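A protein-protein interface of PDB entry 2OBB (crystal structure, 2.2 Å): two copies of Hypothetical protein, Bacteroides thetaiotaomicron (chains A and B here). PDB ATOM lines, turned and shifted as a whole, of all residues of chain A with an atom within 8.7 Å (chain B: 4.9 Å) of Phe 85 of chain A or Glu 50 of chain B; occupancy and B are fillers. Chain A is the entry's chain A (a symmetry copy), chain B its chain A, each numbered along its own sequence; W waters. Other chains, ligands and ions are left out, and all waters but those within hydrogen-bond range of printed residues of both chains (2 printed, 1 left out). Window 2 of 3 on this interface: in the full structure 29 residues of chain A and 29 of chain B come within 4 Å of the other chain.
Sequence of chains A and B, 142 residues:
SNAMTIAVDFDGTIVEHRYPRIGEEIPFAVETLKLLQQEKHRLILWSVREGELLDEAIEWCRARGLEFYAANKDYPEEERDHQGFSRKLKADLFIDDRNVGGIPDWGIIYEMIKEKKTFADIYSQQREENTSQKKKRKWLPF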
ATOM      1  N   TRP A  46     -14.151 -24.934 -28.511  1.00  0.00           N
ATOM      2  CA  TRP A  46     -14.690 -24.639 -27.180  1.00  0.00           C
ATOM      3  C   TRP A  46     -16.138 -24.251 -27.347  1.00  0.00           C
ATOM      4  O   TRP A  46     -16.440 -23.091 -27.644  1.00  0.00           O
ATOM      5  CB  TRP A  46     -13.885 -23.489 -26.571  1.00  0.00           C
ATOM      6  CG  TRP A  46     -14.033 -23.169 -25.100  1.00  0.00           C
ATOM      7  CD1 TRP A  46     -14.006 -21.926 -24.568  1.00  0.00           C
ATOM      8  CD2 TRP A  46     -14.189 -24.084 -23.979  1.00  0.00           C
ATOM      9  NE1 TRP A  46     -14.137 -21.991 -23.202  1.00  0.00           N
ATOM     10  CE2 TRP A  46     -14.247 -23.296 -22.813  1.00  0.00           C
ATOM     11  CE3 TRP A  46     -14.292 -25.477 -23.856  1.00  0.00           C
ATOM     12  CZ2 TRP A  46     -14.373 -23.849 -21.521  1.00  0.00           C
ATOM     13  CZ3 TRP A  46     -14.433 -26.031 -22.588  1.00  0.00           C
ATOM     14  CH2 TRP A  46     -14.467 -25.206 -21.424  1.00  0.00           C
ATOM     15  N   ASN A  72     -13.051 -29.295 -26.570  1.00  0.00           N
ATOM     16  CA  ASN A  72     -13.572 -29.157 -25.214  1.00  0.00           C
ATOM     17  C   ASN A  72     -12.716 -29.923 -24.217  1.00  0.00           C
ATOM     18  O   ASN A  72     -13.200 -30.371 -23.166  1.00  0.00           O
ATOM     19  CB  ASN A  72     -15.051 -29.576 -25.135  1.00  0.00           C
ATOM     20  CG  ASN A  72     -15.955 -28.711 -26.010  1.00  0.00           C
ATOM     21  OD1 ASN A  72     -15.580 -27.602 -26.410  1.00  0.00           O
ATOM     22  ND2 ASN A  72     -17.143 -29.217 -26.319  1.00  0.00           N
ATOM     23  N   LYS A  73     -11.454 -30.102 -24.572  1.00  0.00           N
ATOM     24  CA  LYS A  73     -10.479 -30.617 -23.629  1.00  0.00           C
ATOM     25  C   LYS A  73      -9.233 -29.767 -23.769  1.00  0.00           C
ATOM     26  O   LYS A  73      -9.065 -29.047 -24.775  1.00  0.00           O
ATOM     27  CB  LYS A  73     -10.117 -32.067 -23.936  1.00  0.00           C
ATOM     28  CG  LYS A  73     -11.262 -33.045 -24.138  1.00  0.00           C
ATOM     29  CD  LYS A  73     -10.669 -34.436 -24.362  1.00  0.00           C
ATOM     30  CE  LYS A  73     -11.697 -35.435 -24.833  1.00  0.00           C
ATOM     31  NZ  LYS A  73     -12.955 -35.209 -24.078  1.00  0.00           N
ATOM     32  N   ASP A  74      -8.369 -29.852 -22.765  1.00  0.00           N
ATOM     33  CA  ASP A  74      -7.090 -29.147 -22.785  1.00  0.00           C
ATOM     34  C   ASP A  74      -6.070 -29.868 -23.644  1.00  0.00           C
ATOM     35  O   ASP A  74      -5.094 -29.265 -24.107  1.00  0.00           O
ATOM     36  CB  ASP A  74      -6.556 -28.929 -21.358  1.00  0.00           C
ATOM     37  CG  ASP A  74      -7.111 -27.667 -20.737  1.00  0.00           C
ATOM     38  OD1 ASP A  74      -7.277 -26.677 -21.485  1.00  0.00           O
ATOM     39  OD2 ASP A  74      -7.411 -27.661 -19.526  1.00  0.00           O
ATOM     40  N   TYR A  75      -6.298 -31.158 -23.847  1.00  0.00           N
ATOM     41  CA  TYR A  75      -5.464 -31.978 -24.710  1.00  0.00           C
ATOM     42  C   TYR A  75      -6.220 -33.273 -25.003  1.00  0.00           C
ATOM     43  O   TYR A  75      -6.914 -33.798 -24.126  1.00  0.00           O
ATOM     44  CB  TYR A  75      -4.077 -32.235 -24.090  1.00  0.00           C
ATOM     45  CG  TYR A  75      -4.089 -32.617 -22.625  1.00  0.00           C
ATOM     46  CD1 TYR A  75      -4.236 -33.947 -22.236  1.00  0.00           C
ATOM     47  CD2 TYR A  75      -3.926 -31.652 -21.631  1.00  0.00           C
ATOM     48  CE1 TYR A  75      -4.234 -34.306 -20.901  1.00  0.00           C
ATOM     49  CE2 TYR A  75      -3.922 -32.001 -20.286  1.00  0.00           C
ATOM     50  CZ  TYR A  75      -4.079 -33.333 -19.931  1.00  0.00           C
ATOM     51  OH  TYR A  75      -4.084 -33.701 -18.609  1.00  0.00           O
ATOM     52  N   GLU A  78      -7.746 -36.107 -22.370  1.00  0.00           N
ATOM     53  CA  GLU A  78      -7.921 -35.714 -20.960  1.00  0.00           C
ATOM     54  C   GLU A  78      -8.596 -36.775 -20.080  1.00  0.00           C
ATOM     55  O   GLU A  78      -9.613 -37.366 -20.459  1.00  0.00           O
ATOM     56  CB  GLU A  78      -8.689 -34.398 -20.847  1.00  0.00           C
ATOM     57  CG  GLU A  78      -7.841 -33.156 -21.041  1.00  0.00           C
ATOM     58  CD  GLU A  78      -8.200 -32.057 -20.068  1.00  0.00           C
ATOM     59  OE1 GLU A  78      -7.730 -32.126 -18.901  1.00  0.00           O
ATOM     60  OE2 GLU A  78      -8.938 -31.127 -20.472  1.00  0.00           O
ATOM     61  N   HIS A  82     -10.092 -37.173 -12.313  1.00  0.00           N
ATOM     62  CA  HIS A  82      -9.227 -36.696 -13.388  1.00  0.00           C
ATOM     63  C   HIS A  82      -7.793 -36.434 -12.899  1.00  0.00           C
ATOM     64  O   HIS A  82      -7.336 -37.106 -11.965  1.00  0.00           O
ATOM     65  CB  HIS A  82      -9.856 -35.483 -14.081  1.00  0.00           C
ATOM     66  CG  HIS A  82     -10.798 -35.843 -15.192  1.00  0.00           C
ATOM     67  ND1 HIS A  82     -10.438 -35.778 -16.523  1.00  0.00           N
ATOM     68  CD2 HIS A  82     -12.083 -36.274 -15.171  1.00  0.00           C
ATOM     69  CE1 HIS A  82     -11.462 -36.152 -17.271  1.00  0.00           C
ATOM     70  NE2 HIS A  82     -12.473 -36.456 -16.476  1.00  0.00           N
ATOM     71  N   GLN A  83      -7.087 -35.473 -13.507  1.00  0.00           N
ATOM     72  CA  GLN A  83      -5.625 -35.353 -13.299  1.00  0.00           C
ATOM     73  C   GLN A  83      -5.052 -33.980 -12.845  1.00  0.00           C
ATOM     74  O   GLN A  83      -4.687 -33.813 -11.672  1.00  0.00           O
ATOM     75  CB  GLN A  83      -4.843 -35.966 -14.497  1.00  0.00           C
ATOM     76  CG  GLN A  83      -5.270 -35.504 -15.922  1.00  0.00           C
ATOM     77  CD  GLN A  83      -5.234 -36.629 -16.984  1.00  0.00           C
ATOM     78  OE1 GLN A  83      -4.955 -37.799 -16.675  1.00  0.00           O
ATOM     79  NE2 GLN A  83      -5.532 -36.269 -18.237  1.00  0.00           N
ATOM     80  N   GLY A  84      -4.934 -33.033 -13.778  1.00  0.00           N
ATOM     81  CA  GLY A  84      -4.510 -31.655 -13.482  1.00  0.00           C
ATOM     82  C   GLY A  84      -5.662 -30.756 -13.899  1.00  0.00           C
ATOM     83  O   GLY A  84      -5.473 -29.597 -14.299  1.00  0.00           O
ATOM     84  N   PHE A  85      -6.860 -31.332 -13.764  1.00  0.00           N
ATOM     85  CA  PHE A  85      -8.131 -30.846 -14.308  1.00  0.00           C
ATOM     86  C   PHE A  85      -8.573 -29.482 -13.802  1.00  0.00           C
ATOM     87  O   PHE A  85      -8.331 -29.113 -12.641  1.00  0.00           O
ATOM     88  CB  PHE A  85      -9.237 -31.874 -13.988  1.00  0.00           C
ATOM     89  CG  PHE A  85     -10.452 -31.792 -14.893  1.00  0.00           C
ATOM     90  CD1 PHE A  85     -10.404 -32.269 -16.208  1.00  0.00           C
ATOM     91  CD2 PHE A  85     -11.656 -31.276 -14.425  1.00  0.00           C
ATOM     92  CE1 PHE A  85     -11.529 -32.212 -17.045  1.00  0.00           C
ATOM     93  CE2 PHE A  85     -12.787 -31.217 -15.267  1.00  0.00           C
ATOM     94  CZ  PHE A  85     -12.713 -31.683 -16.576  1.00  0.00           C
ATOM     95  N   SER A  86      -9.205 -28.745 -14.712  1.00  0.00           N
ATOM     96  CA  SER A  86     -10.116 -27.647 -14.383  1.00  0.00           C
ATOM     97  C   SER A  86     -11.252 -27.686 -15.423  1.00  0.00           C
ATOM     98  O   SER A  86     -11.032 -28.076 -16.567  1.00  0.00           O
ATOM     99  CB  SER A  86      -9.382 -26.302 -14.415  1.00  0.00           C
ATOM    100  OG  SER A  86      -8.943 -25.970 -15.736  1.00  0.00           O
ATOM    101  N   ARG A  87     -12.460 -27.302 -15.040  1.00  0.00           N
ATOM    102  CA  ARG A  87     -13.555 -27.295 -15.999  1.00  0.00           C
ATOM    103  C   ARG A  87     -13.329 -26.279 -17.136  1.00  0.00           C
ATOM    104  O   ARG A  87     -13.554 -26.588 -18.310  1.00  0.00           O
ATOM    105  CB  ARG A  87     -14.882 -27.050 -15.291  1.00  0.00           C
ATOM    106  CG  ARG A  87     -16.067 -27.323 -16.162  1.00  0.00           C
ATOM    107  CD  ARG A  87     -17.353 -27.184 -15.392  1.00  0.00           C
ATOM    108  NE  ARG A  87     -18.449 -26.922 -16.317  1.00  0.00           N
ATOM    109  CZ  ARG A  87     -19.734 -26.928 -15.997  1.00  0.00           C
ATOM    110  NH1 ARG A  87     -20.120 -27.172 -14.768  1.00  0.00           N
ATOM    111  NH2 ARG A  87     -20.639 -26.679 -16.925  1.00  0.00           N
ATOM    112  N   LYS A  88     -12.848 -25.086 -16.789  1.00  0.00           N
ATOM    113  CA  LYS A  88     -12.522 -24.068 -17.777  1.00  0.00           C
ATOM    114  C   LYS A  88     -11.192 -24.443 -18.454  1.00  0.00           C
ATOM    115  O   LYS A  88     -10.240 -24.816 -17.774  1.00  0.00           O
ATOM    116  CB  LYS A  88     -12.419 -22.697 -17.082  1.00  0.00           C
ATOM    117  CG  LYS A  88     -12.220 -21.512 -18.007  1.00  0.00           C
ATOM    118  CD  LYS A  88     -12.118 -20.210 -17.214  1.00  0.00           C
ATOM    119  CE  LYS A  88     -11.755 -19.028 -18.106  1.00  0.00           C
ATOM    120  NZ  LYS A  88     -11.254 -17.840 -17.318  1.00  0.00           N
ATOM    121  N   LEU A  89     -11.129 -24.335 -19.776  1.00  0.00           N
ATOM    122  CA  LEU A  89      -9.886 -24.579 -20.509  1.00  0.00           C
ATOM    123  C   LEU A  89      -8.740 -23.709 -20.019  1.00  0.00           C
ATOM    124  O   LEU A  89      -8.949 -22.565 -19.586  1.00  0.00           O
ATOM    125  CB  LEU A  89     -10.060 -24.296 -21.995  1.00  0.00           C
ATOM    126  CG  LEU A  89     -10.953 -25.232 -22.795  1.00  0.00           C
ATOM    127  CD1 LEU A  89     -10.773 -24.942 -24.267  1.00  0.00           C
ATOM    128  CD2 LEU A  89     -10.706 -26.709 -22.469  1.00  0.00           C
ATOM    129  N   LYS A  90      -7.527 -24.230 -20.128  1.00  0.00           N
ATOM    130  CA  LYS A  90      -6.355 -23.450 -19.782  1.00  0.00           C
ATOM    131  C   LYS A  90      -5.796 -22.652 -20.964  1.00  0.00           C
ATOM    132  O   LYS A  90      -4.668 -22.165 -20.887  1.00  0.00           O
ATOM    133  CB  LYS A  90      -5.285 -24.346 -19.165  1.00  0.00           C
ATOM    134  CG  LYS A  90      -5.811 -25.079 -17.960  1.00  0.00           C
ATOM    135  CD  LYS A  90      -4.679 -25.553 -17.042  1.00  0.00           C
ATOM    136  CE  LYS A  90      -5.213 -25.960 -15.693  1.00  0.00           C
ATOM    137  NZ  LYS A  90      -5.881 -27.267 -15.819  1.00  0.00           N
ATOM    138  N   VAL B  48      -9.934 -21.168 -13.979  1.00  0.00           N
ATOM    139  CA  VAL B  48      -9.246 -22.443 -13.969  1.00  0.00           C
ATOM    140  C   VAL B  48      -8.990 -22.880 -12.519  1.00  0.00           C
ATOM    141  O   VAL B  48      -8.695 -24.046 -12.274  1.00  0.00           O
ATOM    142  CB  VAL B  48      -7.925 -22.447 -14.822  1.00  0.00           C
ATOM    143  CG1 VAL B  48      -8.248 -22.278 -16.310  1.00  0.00           C
ATOM    144  CG2 VAL B  48      -6.920 -21.387 -14.324  1.00  0.00           C
ATOM    145  N   ARG B  49      -9.112 -21.944 -11.571  1.00  0.00           N
ATOM    146  CA  ARG B  49      -9.056 -22.268 -10.135  1.00  0.00           C
ATOM    147  C   ARG B  49     -10.084 -23.362  -9.766  1.00  0.00           C
ATOM    148  O   ARG B  49     -11.266 -23.285 -10.165  1.00  0.00           O
ATOM    149  CB  ARG B  49      -9.292 -21.012  -9.278  1.00  0.00           C
ATOM    150  CG  ARG B  49      -8.108 -20.040  -9.235  1.00  0.00           C
ATOM    151  CD  ARG B  49      -8.438 -18.725  -8.504  1.00  0.00           C
ATOM    152  NE  ARG B  49      -7.309 -17.787  -8.473  1.00  0.00           N
ATOM    153  CZ  ARG B  49      -6.507 -17.573  -7.427  1.00  0.00           C
ATOM    154  NH1 ARG B  49      -6.687 -18.221  -6.279  1.00  0.00           N
ATOM    155  NH2 ARG B  49      -5.507 -16.697  -7.528  1.00  0.00           N
ATOM    156  N   GLU B  50      -9.610 -24.371  -9.034  1.00  0.00           N
ATOM    157  CA  GLU B  50     -10.431 -25.427  -8.417  1.00  0.00           C
ATOM    158  C   GLU B  50      -9.964 -25.664  -6.957  1.00  0.00           C
ATOM    159  O   GLU B  50      -8.858 -25.275  -6.573  1.00  0.00           O
ATOM    160  CB  GLU B  50     -10.289 -26.765  -9.167  1.00  0.00           C
ATOM    161  CG  GLU B  50     -10.538 -26.751 -10.682  1.00  0.00           C
ATOM    162  CD  GLU B  50     -12.034 -26.724 -11.088  1.00  0.00           C
ATOM    163  OE1 GLU B  50     -12.940 -26.538 -10.220  1.00  0.00           O
ATOM    164  OE2 GLU B  50     -12.294 -26.886 -12.301  1.00  0.00           O
ATOM    165  N   GLY B  51     -10.792 -26.319  -6.149  1.00  0.00           N
ATOM    166  CA  GLY B  51     -10.393 -26.661  -4.778  1.00  0.00           C
ATOM    167  C   GLY B  51     -10.107 -25.427  -3.952  1.00  0.00           C
ATOM    168  O   GLY B  51     -10.773 -24.387  -4.126  1.00  0.00           O
ATOM    169  N   GLU B  52      -9.121 -25.512  -3.060  1.00  0.00           N
ATOM    170  CA  GLU B  52      -8.844 -24.411  -2.128  1.00  0.00           C
ATOM    171  C   GLU B  52      -8.381 -23.097  -2.789  1.00  0.00           C
ATOM    172  O   GLU B  52      -8.542 -22.025  -2.196  1.00  0.00           O
ATOM    173  CB  GLU B  52      -7.899 -24.848  -0.999  1.00  0.00           C
ATOM    174  CG  GLU B  52      -8.595 -25.595   0.173  1.00  0.00           C
ATOM    175  CD  GLU B  52      -9.294 -24.658   1.180  1.00  0.00           C
ATOM    176  OE1 GLU B  52      -8.708 -24.389   2.247  1.00  0.00           O
ATOM    177  OE2 GLU B  52     -10.422 -24.190   0.912  1.00  0.00           O
ATOM    178  N   LEU B  53      -7.831 -23.170  -4.001  1.00  0.00           N
ATOM    179  CA  LEU B  53      -7.509 -21.949  -4.754  1.00  0.00           C
ATOM    180  C   LEU B  53      -8.756 -21.230  -5.274  1.00  0.00           C
ATOM    181  O   LEU B  53      -8.791 -19.997  -5.335  1.00  0.00           O
ATOM    182  CB  LEU B  53      -6.539 -22.243  -5.894  1.00  0.00           C
ATOM    183  CG  LEU B  53      -5.103 -22.536  -5.455  1.00  0.00           C
ATOM    184  CD1 LEU B  53      -4.240 -22.900  -6.666  1.00  0.00           C
ATOM    185  CD2 LEU B  53      -4.506 -21.361  -4.669  1.00  0.00           C
ATOM    186  N   LEU B  54      -9.773 -22.003  -5.646  1.00  0.00           N
ATOM    187  CA  LEU B  54     -11.082 -21.446  -5.929  1.00  0.00           C
ATOM    188  C   LEU B  54     -11.675 -20.829  -4.669  1.00  0.00           C
ATOM    189  O   LEU B  54     -12.129 -19.681  -4.683  1.00  0.00           O
ATOM    190  CB  LEU B  54     -12.037 -22.510  -6.485  1.00  0.00           C
ATOM    191  CG  LEU B  54     -13.376 -22.010  -7.084  1.00  0.00           C
ATOM    192  CD1 LEU B  54     -13.177 -20.985  -8.244  1.00  0.00           C
ATOM    193  CD2 LEU B  54     -14.266 -23.199  -7.522  1.00  0.00           C
ATOM    194  N   ASN B  72     -18.021 -21.804 -11.469  1.00  0.00           N
ATOM    195  CA  ASN B  72     -17.624 -22.835 -12.423  1.00  0.00           C
ATOM    196  C   ASN B  72     -18.727 -23.864 -12.611  1.00  0.00           C
ATOM    197  O   ASN B  72     -18.466 -25.033 -12.934  1.00  0.00           O
ATOM    198  CB  ASN B  72     -16.293 -23.493 -12.017  1.00  0.00           C
ATOM    199  CG  ASN B  72     -15.134 -22.502 -11.978  1.00  0.00           C
ATOM    200  OD1 ASN B  72     -15.206 -21.416 -12.567  1.00  0.00           O
ATOM    201  ND2 ASN B  72     -14.065 -22.864 -11.278  1.00  0.00           N
ATOM    202  N   ARG B  87     -19.317 -28.906 -20.698  1.00  0.00           N
ATOM    203  CA  ARG B  87     -18.157 -28.441 -19.951  1.00  0.00           C
ATOM    204  C   ARG B  87     -18.031 -26.905 -19.964  1.00  0.00           C
ATOM    205  O   ARG B  87     -17.763 -26.287 -18.929  1.00  0.00           O
ATOM    206  CB  ARG B  87     -16.888 -29.107 -20.470  1.00  0.00           C
ATOM    207  CG  ARG B  87     -15.713 -28.906 -19.566  1.00  0.00           C
ATOM    208  CD  ARG B  87     -14.514 -29.675 -20.052  1.00  0.00           C
ATOM    209  NE  ARG B  87     -13.299 -29.074 -19.516  1.00  0.00           N
ATOM    210  CZ  ARG B  87     -12.088 -29.603 -19.594  1.00  0.00           C
ATOM    211  NH1 ARG B  87     -11.894 -30.752 -20.196  1.00  0.00           N
ATOM    212  NH2 ARG B  87     -11.060 -28.965 -19.066  1.00  0.00           N
HETATM  213  O   HOH W   1     -18.381 -27.990 -23.317  1.00  0.00           O
HETATM  214  O   HOH W   2      -8.914 -18.774 -15.508  1.00  0.00           O
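Of chain B, only Glu 50 (3.8 Å) and Arg 87 (3.5 Å) come within 4 Å of Phe 85 of chain A. Printed residues of chain B within 4 Å of Arg 87 of chain A: Glu 50, Asn 72 and Arg 87. Of chain A, only Phe 85 (3.8 Å), Ser 86 (3.1 Å) and Arg 87 (2.8 Å) come within 4 Å of Glu 50 of chain B. No residue of chain A comes within 4 Å of Gly 51 of chain B. Of the printed residues of chain A, Arg 87 of chain B touches Asn 72, Lys 73, Asp 74, Glu 78, Phe 85, Ser 86 and Arg 87. The nearest residue of chain A that does not touch Glu 50 of chain B is Lys 88 of chain A (4.9 Å). The nearest printed residue of chain B that does not touch Asn 72 of chain A is Glu 50 of chain B (11.4 Å).
Water W1 bridges the backbone NH of Arg 87 of chain B (2.9 Å) and the side-chain amide nitrogen of Asn 72 of chain A (3.5 Å). Water W2 bridges N of Val 48 of chain B (3.0 Å) and NZ of Lys 88 of chain A (3.1 Å).
N of Arg 87 of chain A sits at hydrogen-bond distance from OE2 of Glu 50 of chain B (2.8 Å). NH1 of Arg 87 of chain A lies within hydrogen-bond range of O of Asn 72 of chain B. The backbone carbonyl oxygen of Asn 72 of chain A lies within hydrogen-bond range of the guanidinium group of Arg 87 of chain B, 3.3 Å away. OD2 of Asp 74 of chain A is in salt-bridge range of NH2 of Arg 87 of chain B (3.9 Å). The guanidinium group of Arg 87 of chain B lies within salt-bridge range of the side-chain carboxylate of Glu 78 of chain A (3.0 Å). The backbone carbonyl oxygen of Ser 86 of chain A is in hydrogen-bond range of the guanidinium group of Arg 87 of chain B (2.7 Å). The guanidinium group of Arg 87 of chain B is in hydrogen-bond range of the backbone carbonyl oxygen of Arg 87 of chain A (2.8 Å).
O of Arg 49 of chain B is in hydrogen-bond range of ND2 of Asn 72 of chain B, 3.0 Å away. OE2 of Glu 78 of chain A is in hydrogen-bond range of N of Asp 74 of chain A. The backbone NH (N) of Lys 90 of chain A sits at hydrogen-bond distance from the side-chain carboxylate (OD1) of Asp 74 of chain A (2.8 Å). The side-chain hydroxyl of Ser 86 of chain A sits at hydrogen-bond distance from the backbone carbonyl oxygen of Lys 88 of chain A (2.7 Å). The side-chain amino group of Lys 90 of chain A is in hydrogen-bond range of the side-chain hydroxyl of Ser 86 of chain A (3.3 Å).
Hydrophobic or aromatic side chains of chain A within 4 Å of the printed part of chain B: Phe 85. Printed residues of chain B that touch a printed residue of chain A: Val 48, Glu 50, Asn 72 and Arg 87. Hydrophobic or aromatic side chains of chain B within 4 Å of the printed part of chain A: Val 48. Among the printed residues, Asp or Glu carboxylates within 4 Å of a Lys or Arg side-chain nitrogen of the other chain: Asp 74 of chain A with Arg 87 of chain B (3.9 Å) and Glu 78 of chain A with Arg 87 of chain B (3.0 Å).
Asn 72 of chain A touches Arg 87 of chain B, and with the chains exchanged Arg 87 of chain A touches Asn 72 of chain B. Arg 87 of chain A touches its own counterpart, Arg 87 of chain B. 2 positions are printed for both chains. Of the 14 pairs that touch across the chains among the printed residues, 3 have their exchanged pair printed and touching as well.
Among the printed residues, merely in contact across the chains: Lys 73 of chain A with Arg 87 of chain B (3.7 Å), Phe 85 of chain A with Glu 50 of chain B (3.8 Å), Phe 85 of chain A with Arg 87 of chain B (3.5 Å), Ser 86 of chain A with Val 48 of chain B (3.2 Å), Ser 86 of chain A with Glu 50 of chain B (3.1 Å), Lys 88 of chain A with Val 48 of chain B (3.5 Å) and Leu 89 of chain A with Val 48 of chain B (3.4 Å).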
